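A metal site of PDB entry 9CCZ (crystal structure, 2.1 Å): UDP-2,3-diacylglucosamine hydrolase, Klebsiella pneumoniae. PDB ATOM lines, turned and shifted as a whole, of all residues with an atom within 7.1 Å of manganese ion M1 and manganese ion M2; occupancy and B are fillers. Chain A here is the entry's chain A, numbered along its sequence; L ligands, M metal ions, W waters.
ND2 of Asn 79 lies within hydrogen-bond range of O3 of the ligand (3.0 Å).
The backbone NH (N) of His 195 sits at hydrogen-bond distance from the side-chain carboxylate (OD2) of Asp 8 (2.7 Å).
The backbone NH (N) of Asp 8 lies within hydrogen-bond range of the backbone carbonyl oxygen (O) of Gly 40, 3.0 Å away.
The backbone carbonyl oxygen (O) of His 114 is in hydrogen-bond range of the backbone NH (N) of Gly 194 (2.8 Å).
The backbone carbonyl oxygen (O) of Leu 39 sits at hydrogen-bond distance from a ring nitrogen (ND1) of His 114 (2.8 Å).
The backbone NH (N) of Arg 80 lies within hydrogen-bond range of the side-chain carboxylate (OD1) of Asp 41, 3.0 Å away.
O of Asp 41 lies within hydrogen-bond range of N of Leu 9.
The side-chain carboxylate of Glu 44 lies within hydrogen-bond range of a ring nitrogen (ND1) of His 10, at 2.8 Å.
Of the 22 residues printed, 5 come within 4 Å of manganese ion M1.
The nearest printed residue that does not touch manganese ion M1 is His 197 (5.1 Å).
Within 4 Å of manganese ion M2: Asp 8, His 10, Asp 41 and His 197.
The nearest printed residue that does not touch manganese ion M2 is His 195 (4.001 Å).
Manganese ion M1 is bound by OD1 of Asn 79 (1.9 Å), water W2 (1.9 Å), NE2 of His 114 (2.1 Å), OD2 of Asp 41 (2.2 Å) and ND1 of His 195 (2.3 Å).
Manganese ion M2 is bound by water W2, the side-chain carboxylate (OD1) of Asp 8, a ring nitrogen (NE2) of His 197, a ring nitrogen (NE2) of His 10 and the side-chain carboxylate (OD2) of Asp 41.
Manganese ion M2 has five donor atoms within binding distance.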
ATOM      1  N   ALA A   7     -26.547 -24.330 -11.100  1.00  0.00           N
ATOM      2  CA  ALA A   7     -25.372 -23.680 -11.693  1.00  0.00           C
ATOM      3  C   ALA A   7     -24.174 -23.905 -10.780  1.00  0.00           C
ATOM      4  O   ALA A   7     -24.314 -24.305  -9.621  1.00  0.00           O
ATOM      5  CB  ALA A   7     -25.595 -22.180 -11.922  1.00  0.00           C
ATOM      6  N   ASP A   8     -22.989 -23.645 -11.330  1.00  0.00           N
ATOM      7  CA  ASP A   8     -21.748 -23.586 -10.557  1.00  0.00           C
ATOM      8  C   ASP A   8     -21.502 -24.884  -9.802  1.00  0.00           C
ATOM      9  O   ASP A   8     -21.127 -24.878  -8.625  1.00  0.00           O
ATOM     10  CB  ASP A   8     -21.763 -22.379  -9.618  1.00  0.00           C
ATOM     11  CG  ASP A   8     -21.865 -21.077 -10.371  1.00  0.00           C
ATOM     12  OD1 ASP A   8     -20.891 -20.738 -11.082  1.00  0.00           O
ATOM     13  OD2 ASP A   8     -22.913 -20.415 -10.295  1.00  0.00           O
ATOM     14  N   LEU A   9     -21.711 -26.006 -10.483  1.00  0.00           N
ATOM     15  CA  LEU A   9     -21.318 -27.300  -9.925  1.00  0.00           C
ATOM     16  C   LEU A   9     -19.804 -27.492  -9.979  1.00  0.00           C
ATOM     17  O   LEU A   9     -19.238 -28.148  -9.102  1.00  0.00           O
ATOM     18  CB  LEU A   9     -22.038 -28.423 -10.667  1.00  0.00           C
ATOM     19  CG  LEU A   9     -23.525 -28.602 -10.357  1.00  0.00           C
ATOM     20  CD1 LEU A   9     -24.392 -27.655 -11.181  1.00  0.00           C
ATOM     21  CD2 LEU A   9     -23.934 -30.042 -10.582  1.00  0.00           C
ATOM     22  N   HIS A  10     -19.147 -26.912 -10.977  1.00  0.00           N
ATOM     23  CA  HIS A  10     -17.699 -27.025 -11.153  1.00  0.00           C
ATOM     24  C   HIS A  10     -17.247 -28.489 -11.054  1.00  0.00           C
ATOM     25  O   HIS A  10     -16.307 -28.825 -10.320  1.00  0.00           O
ATOM     26  CB  HIS A  10     -16.951 -26.160 -10.135  1.00  0.00           C
ATOM     27  CG  HIS A  10     -17.249 -24.695 -10.240  1.00  0.00           C
ATOM     28  ND1 HIS A  10     -16.448 -23.826 -10.957  1.00  0.00           N
ATOM     29  CD2 HIS A  10     -18.261 -23.948  -9.734  1.00  0.00           C
ATOM     30  CE1 HIS A  10     -16.958 -22.608 -10.869  1.00  0.00           C
ATOM     31  NE2 HIS A  10     -18.051 -22.655 -10.138  1.00  0.00           N
ATOM     32  N   LEU A  39     -27.360 -23.128 -15.562  1.00  0.00           N
ATOM     33  CA  LEU A  39     -26.936 -21.766 -15.895  1.00  0.00           C
ATOM     34  C   LEU A  39     -25.424 -21.585 -15.784  1.00  0.00           C
ATOM     35  O   LEU A  39     -24.949 -20.618 -15.193  1.00  0.00           O
ATOM     36  CB  LEU A  39     -27.673 -20.765 -15.008  1.00  0.00           C
ATOM     37  CG  LEU A  39     -29.202 -20.838 -15.013  1.00  0.00           C
ATOM     38  CD1 LEU A  39     -29.809 -19.667 -14.244  1.00  0.00           C
ATOM     39  CD2 LEU A  39     -29.746 -20.890 -16.429  1.00  0.00           C
ATOM     40  N   GLY A  40     -24.656 -22.521 -16.331  1.00  0.00           N
ATOM     41  CA  GLY A  40     -23.235 -22.295 -16.522  1.00  0.00           C
ATOM     42  C   GLY A  40     -22.390 -22.828 -15.376  1.00  0.00           C
ATOM     43  O   GLY A  40     -22.860 -23.031 -14.249  1.00  0.00           O
ATOM     44  N   ASP A  41     -21.107 -23.032 -15.679  1.00  0.00           N
ATOM     45  CA  ASP A  41     -20.143 -23.616 -14.750  1.00  0.00           C
ATOM     46  C   ASP A  41     -20.601 -24.992 -14.275  1.00  0.00           C
ATOM     47  O   ASP A  41     -20.438 -25.359 -13.105  1.00  0.00           O
ATOM     48  CB  ASP A  41     -19.877 -22.694 -13.560  1.00  0.00           C
ATOM     49  CG  ASP A  41     -19.039 -21.482 -13.931  1.00  0.00           C
ATOM     50  OD1 ASP A  41     -18.643 -21.361 -15.122  1.00  0.00           O
ATOM     51  OD2 ASP A  41     -18.762 -20.647 -13.040  1.00  0.00           O
ATOM     52  N   GLU A  44     -15.732 -27.546 -14.091  1.00  0.00           N
ATOM     53  CA  GLU A  44     -14.669 -26.641 -13.668  1.00  0.00           C
ATOM     54  C   GLU A  44     -13.841 -26.162 -14.852  1.00  0.00           C
ATOM     55  O   GLU A  44     -13.262 -25.073 -14.804  1.00  0.00           O
ATOM     56  CB  GLU A  44     -13.778 -27.331 -12.637  1.00  0.00           C
ATOM     57  CG  GLU A  44     -12.509 -26.562 -12.245  1.00  0.00           C
ATOM     58  CD  GLU A  44     -12.795 -25.248 -11.521  1.00  0.00           C
ATOM     59  OE1 GLU A  44     -13.949 -25.005 -11.132  1.00  0.00           O
ATOM     60  OE2 GLU A  44     -11.851 -24.446 -11.362  1.00  0.00           O
ATOM     61  N   GLY A  78     -21.165 -20.920 -18.781  1.00  0.00           N
ATOM     62  CA  GLY A  78     -20.506 -20.172 -17.738  1.00  0.00           C
ATOM     63  C   GLY A  78     -19.149 -19.671 -18.186  1.00  0.00           C
ATOM     64  O   GLY A  78     -18.741 -19.836 -19.335  1.00  0.00           O
ATOM     65  N   ASN A  79     -18.430 -19.048 -17.245  1.00  0.00           N
ATOM     66  CA  ASN A  79     -17.091 -18.578 -17.559  1.00  0.00           C
ATOM     67  C   ASN A  79     -16.065 -19.705 -17.585  1.00  0.00           C
ATOM     68  O   ASN A  79     -15.015 -19.550 -18.221  1.00  0.00           O
ATOM     69  CB  ASN A  79     -16.659 -17.485 -16.561  1.00  0.00           C
ATOM     70  CG  ASN A  79     -16.695 -17.950 -15.121  1.00  0.00           C
ATOM     71  OD1 ASN A  79     -17.765 -18.220 -14.575  1.00  0.00           O
ATOM     72  ND2 ASN A  79     -15.539 -18.019 -14.489  1.00  0.00           N
ATOM     73  N   ARG A  80     -16.348 -20.830 -16.938  1.00  0.00           N
ATOM     74  CA  ARG A  80     -15.424 -21.949 -16.954  1.00  0.00           C
ATOM     75  C   ARG A  80     -15.635 -22.856 -18.165  1.00  0.00           C
ATOM     76  O   ARG A  80     -14.654 -23.359 -18.731  1.00  0.00           O
ATOM     77  CB  ARG A  80     -15.575 -22.769 -15.669  1.00  0.00           C
ATOM     78  CG  ARG A  80     -15.447 -21.962 -14.386  1.00  0.00           C
ATOM     79  CD  ARG A  80     -14.089 -21.311 -14.265  1.00  0.00           C
ATOM     80  NE  ARG A  80     -13.006 -22.295 -14.228  1.00  0.00           N
ATOM     81  CZ  ARG A  80     -11.749 -22.019 -13.914  1.00  0.00           C
ATOM     82  NH1 ARG A  80     -11.372 -20.799 -13.578  1.00  0.00           N
ATOM     83  NH2 ARG A  80     -10.848 -22.998 -13.919  1.00  0.00           N
ATOM     84  N   HIS A 114     -25.764 -16.672 -16.750  1.00  0.00           N
ATOM     85  CA  HIS A 114     -24.785 -17.176 -15.803  1.00  0.00           C
ATOM     86  C   HIS A 114     -24.488 -16.136 -14.725  1.00  0.00           C
ATOM     87  O   HIS A 114     -24.324 -16.479 -13.553  1.00  0.00           O
ATOM     88  CB  HIS A 114     -23.502 -17.588 -16.518  1.00  0.00           C
ATOM     89  CG  HIS A 114     -22.434 -18.067 -15.578  1.00  0.00           C
ATOM     90  ND1 HIS A 114     -22.591 -19.186 -14.787  1.00  0.00           N
ATOM     91  CD2 HIS A 114     -21.211 -17.566 -15.283  1.00  0.00           C
ATOM     92  CE1 HIS A 114     -21.509 -19.354 -14.047  1.00  0.00           C
ATOM     93  NE2 HIS A 114     -20.657 -18.384 -14.333  1.00  0.00           N
ATOM     94  N   GLY A 115     -24.412 -14.864 -15.122  1.00  0.00           N
ATOM     95  CA  GLY A 115     -24.199 -13.771 -14.186  1.00  0.00           C
ATOM     96  C   GLY A 115     -22.864 -13.077 -14.327  1.00  0.00           C
ATOM     97  O   GLY A 115     -22.697 -11.993 -13.740  1.00  0.00           O
ATOM     98  N   ASP A 116     -21.913 -13.646 -15.065  1.00  0.00           N
ATOM     99  CA  ASP A 116     -20.585 -13.039 -15.127  1.00  0.00           C
ATOM    100  C   ASP A 116     -20.598 -11.731 -15.912  1.00  0.00           C
ATOM    101  O   ASP A 116     -19.749 -10.861 -15.669  1.00  0.00           O
ATOM    102  CB  ASP A 116     -19.571 -14.009 -15.726  1.00  0.00           C
ATOM    103  CG  ASP A 116     -19.912 -14.406 -17.151  1.00  0.00           C
ATOM    104  OD1 ASP A 116     -21.062 -14.812 -17.399  1.00  0.00           O
ATOM    105  OD2 ASP A 116     -19.023 -14.292 -18.028  1.00  0.00           O
ATOM    106  N   TYR A 125     -11.129  -9.402 -15.456  1.00  0.00           N
ATOM    107  CA  TYR A 125     -11.896 -10.539 -15.943  1.00  0.00           C
ATOM    108  C   TYR A 125     -12.563 -10.230 -17.281  1.00  0.00           C
ATOM    109  O   TYR A 125     -12.559 -11.078 -18.190  1.00  0.00           O
ATOM    110  CB  TYR A 125     -12.965 -10.963 -14.932  1.00  0.00           C
ATOM    111  CG  TYR A 125     -13.978 -11.878 -15.561  1.00  0.00           C
ATOM    112  CD1 TYR A 125     -13.632 -13.162 -15.943  1.00  0.00           C
ATOM    113  CD2 TYR A 125     -15.275 -11.443 -15.810  1.00  0.00           C
ATOM    114  CE1 TYR A 125     -14.543 -14.011 -16.545  1.00  0.00           C
ATOM    115  CE2 TYR A 125     -16.201 -12.284 -16.411  1.00  0.00           C
ATOM    116  CZ  TYR A 125     -15.831 -13.561 -16.777  1.00  0.00           C
ATOM    117  OH  TYR A 125     -16.744 -14.403 -17.373  1.00  0.00           O
ATOM    118  N   ILE A 171     -14.324 -14.033  -6.122  1.00  0.00           N
ATOM    119  CA  ILE A 171     -15.176 -13.649  -7.242  1.00  0.00           C
ATOM    120  C   ILE A 171     -15.816 -12.296  -6.968  1.00  0.00           C
ATOM    121  O   ILE A 171     -16.434 -12.098  -5.919  1.00  0.00           O
ATOM    122  CB  ILE A 171     -16.241 -14.717  -7.521  1.00  0.00           C
ATOM    123  CG1 ILE A 171     -15.595 -16.083  -7.794  1.00  0.00           C
ATOM    124  CG2 ILE A 171     -17.121 -14.307  -8.700  1.00  0.00           C
ATOM    125  CD1 ILE A 171     -16.551 -17.242  -7.692  1.00  0.00           C
ATOM    126  N   GLY A 194     -26.125 -17.241 -11.529  1.00  0.00           N
ATOM    127  CA  GLY A 194     -25.182 -17.835 -10.609  1.00  0.00           C
ATOM    128  C   GLY A 194     -23.871 -17.062 -10.593  1.00  0.00           C
ATOM    129  O   GLY A 194     -23.872 -15.842 -10.364  1.00  0.00           O
ATOM    130  N   HIS A 195     -22.769 -17.774 -10.837  1.00  0.00           N
ATOM    131  CA  HIS A 195     -21.421 -17.215 -10.981  1.00  0.00           C
ATOM    132  C   HIS A 195     -20.843 -16.660  -9.676  1.00  0.00           C
ATOM    133  O   HIS A 195     -19.697 -16.964  -9.324  1.00  0.00           O
ATOM    134  CB  HIS A 195     -21.373 -16.117 -12.041  1.00  0.00           C
ATOM    135  CG  HIS A 195     -20.018 -15.530 -12.236  1.00  0.00           C
ATOM    136  ND1 HIS A 195     -18.959 -16.255 -12.741  1.00  0.00           N
ATOM    137  CD2 HIS A 195     -19.522 -14.295 -11.969  1.00  0.00           C
ATOM    138  CE1 HIS A 195     -17.884 -15.497 -12.789  1.00  0.00           C
ATOM    139  NE2 HIS A 195     -18.193 -14.296 -12.323  1.00  0.00           N
ATOM    140  N   THR A 196     -21.609 -15.850  -8.949  1.00  0.00           N
ATOM    141  CA  THR A 196     -21.061 -15.176  -7.774  1.00  0.00           C
ATOM    142  C   THR A 196     -20.957 -16.081  -6.554  1.00  0.00           C
ATOM    143  O   THR A 196     -20.293 -15.701  -5.581  1.00  0.00           O
ATOM    144  CB  THR A 196     -21.908 -13.948  -7.428  1.00  0.00           C
ATOM    145  OG1 THR A 196     -23.235 -14.370  -7.075  1.00  0.00           O
ATOM    146  CG2 THR A 196     -21.977 -12.998  -8.612  1.00  0.00           C
ATOM    147  N   HIS A 197     -21.591 -17.256  -6.574  1.00  0.00           N
ATOM    148  CA  HIS A 197     -21.528 -18.208  -5.454  1.00  0.00           C
ATOM    149  C   HIS A 197     -22.049 -17.606  -4.156  1.00  0.00           C
ATOM    150  O   HIS A 197     -21.612 -17.982  -3.064  1.00  0.00           O
ATOM    151  CB  HIS A 197     -20.101 -18.748  -5.266  1.00  0.00           C
ATOM    152  CG  HIS A 197     -19.543 -19.454  -6.468  1.00  0.00           C
ATOM    153  ND1 HIS A 197     -18.319 -20.079  -6.459  1.00  0.00           N
ATOM    154  CD2 HIS A 197     -20.055 -19.649  -7.706  1.00  0.00           C
ATOM    155  CE1 HIS A 197     -18.093 -20.622  -7.634  1.00  0.00           C
ATOM    156  NE2 HIS A 197     -19.129 -20.375  -8.413  1.00  0.00           N
ATOM    157  N   ALA A 218     -22.969 -22.301  -5.325  1.00  0.00           N
ATOM    158  CA  ALA A 218     -22.034 -23.276  -5.858  1.00  0.00           C
ATOM    159  C   ALA A 218     -22.104 -24.564  -5.054  1.00  0.00           C
ATOM    160  O   ALA A 218     -22.395 -24.557  -3.850  1.00  0.00           O
ATOM    161  CB  ALA A 218     -20.602 -22.727  -5.831  1.00  0.00           C
ATOM    162  N   HIS A 220     -20.239 -26.653  -3.315  1.00  0.00           N
ATOM    163  CA  HIS A 220     -18.983 -26.853  -2.601  1.00  0.00           C
ATOM    164  C   HIS A 220     -19.118 -27.980  -1.577  1.00  0.00           C
ATOM    165  O   HIS A 220     -18.413 -28.988  -1.650  1.00  0.00           O
ATOM    166  CB  HIS A 220     -18.541 -25.546  -1.928  1.00  0.00           C
ATOM    167  CG  HIS A 220     -17.980 -24.526  -2.875  1.00  0.00           C
ATOM    168  ND1 HIS A 220     -18.178 -23.179  -2.717  1.00  0.00           N
ATOM    169  CD2 HIS A 220     -17.221 -24.673  -3.982  1.00  0.00           C
ATOM    170  CE1 HIS A 220     -17.570 -22.524  -3.692  1.00  0.00           C
ATOM    171  NE2 HIS A 220     -16.979 -23.407  -4.475  1.00  0.00           N
HETATM  172  N1  LIG L   1      -8.962 -21.980 -22.712  1.00  0.00           N
HETATM  173  C1  LIG L   1      -7.930 -22.637 -21.935  1.00  0.00           C
HETATM  174  C2  LIG L   1     -10.242 -22.660 -22.592  1.00  0.00           C
HETATM  175  C3  LIG L   1     -10.432 -22.022 -17.891  1.00  0.00           C
HETATM  176  C4  LIG L   1      -9.362 -21.317 -17.339  1.00  0.00           C
HETATM  177  C5  LIG L   1     -10.880 -19.554 -16.681  1.00  0.00           C
HETATM  178  C6  LIG L   1     -11.726 -21.496 -17.859  1.00  0.00           C
HETATM  179  C7  LIG L   1     -11.970 -17.350 -15.775  1.00  0.00           C
HETATM  180  C8  LIG L   1      -9.536 -20.055 -25.652  1.00  0.00           C
HETATM  181  C9  LIG L   1      -8.692 -21.124 -23.829  1.00  0.00           C
HETATM  182  C10 LIG L   1      -7.430 -20.631 -24.061  1.00  0.00           C
HETATM  183  C11 LIG L   1      -7.225 -19.818 -25.157  1.00  0.00           C
HETATM  184  C12 LIG L   1      -8.300 -19.508 -25.978  1.00  0.00           C
HETATM  185  C13 LIG L   1      -5.831 -19.257 -25.456  1.00  0.00           C
HETATM  186  C14 LIG L   1      -8.359 -22.615 -20.474  1.00  0.00           C
HETATM  187  C15 LIG L   1     -10.679 -22.681 -21.143  1.00  0.00           C
HETATM  188  C16 LIG L   1      -9.599 -20.079 -16.718  1.00  0.00           C
HETATM  189  C17 LIG L   1     -11.952 -20.270 -17.252  1.00  0.00           C
HETATM  190  C18 LIG L   1     -11.760 -16.032 -15.032  1.00  0.00           C
HETATM  191  C19 LIG L   1      -9.487 -17.981 -15.519  1.00  0.00           C
HETATM  192  C20 LIG L   1      -8.640 -19.112 -16.039  1.00  0.00           C
HETATM  193  F1  LIG L   1      -5.765 -17.960 -25.108  1.00  0.00           F
HETATM  194  F2  LIG L   1      -5.575 -19.381 -26.769  1.00  0.00           F
HETATM  195  F3  LIG L   1      -4.906 -19.951 -24.761  1.00  0.00           F
HETATM  196  N2  LIG L   1      -9.697 -20.825 -24.617  1.00  0.00           N
HETATM  197  N3  LIG L   1      -9.651 -23.243 -20.274  1.00  0.00           N
HETATM  198  N4  LIG L   1     -10.846 -18.243 -15.978  1.00  0.00           N
HETATM  199  O1  LIG L   1     -11.337 -24.441 -18.717  1.00  0.00           O
HETATM  200  O2  LIG L   1      -9.139 -24.414 -17.980  1.00  0.00           O
HETATM  201  O3  LIG L   1     -13.044 -17.648 -16.191  1.00  0.00           O
HETATM  202  S1  LIG L   1     -10.130 -23.605 -18.694  1.00  0.00           S
HETATM  203 CL1  LIG L   1     -10.964 -19.719 -26.657  1.00  0.00          CL
HETATM  204 MN    MN M   1     -18.919 -18.484 -13.097  1.00  0.00          MN
HETATM  205 MN    MN M   2     -19.015 -20.678 -10.646  1.00  0.00          MN
HETATM  206  O   HOH W   1     -15.889 -19.238 -11.645  1.00  0.00           O
HETATM  207  O   HOH W   2     -18.509 -19.073 -11.287  1.00  0.00           O
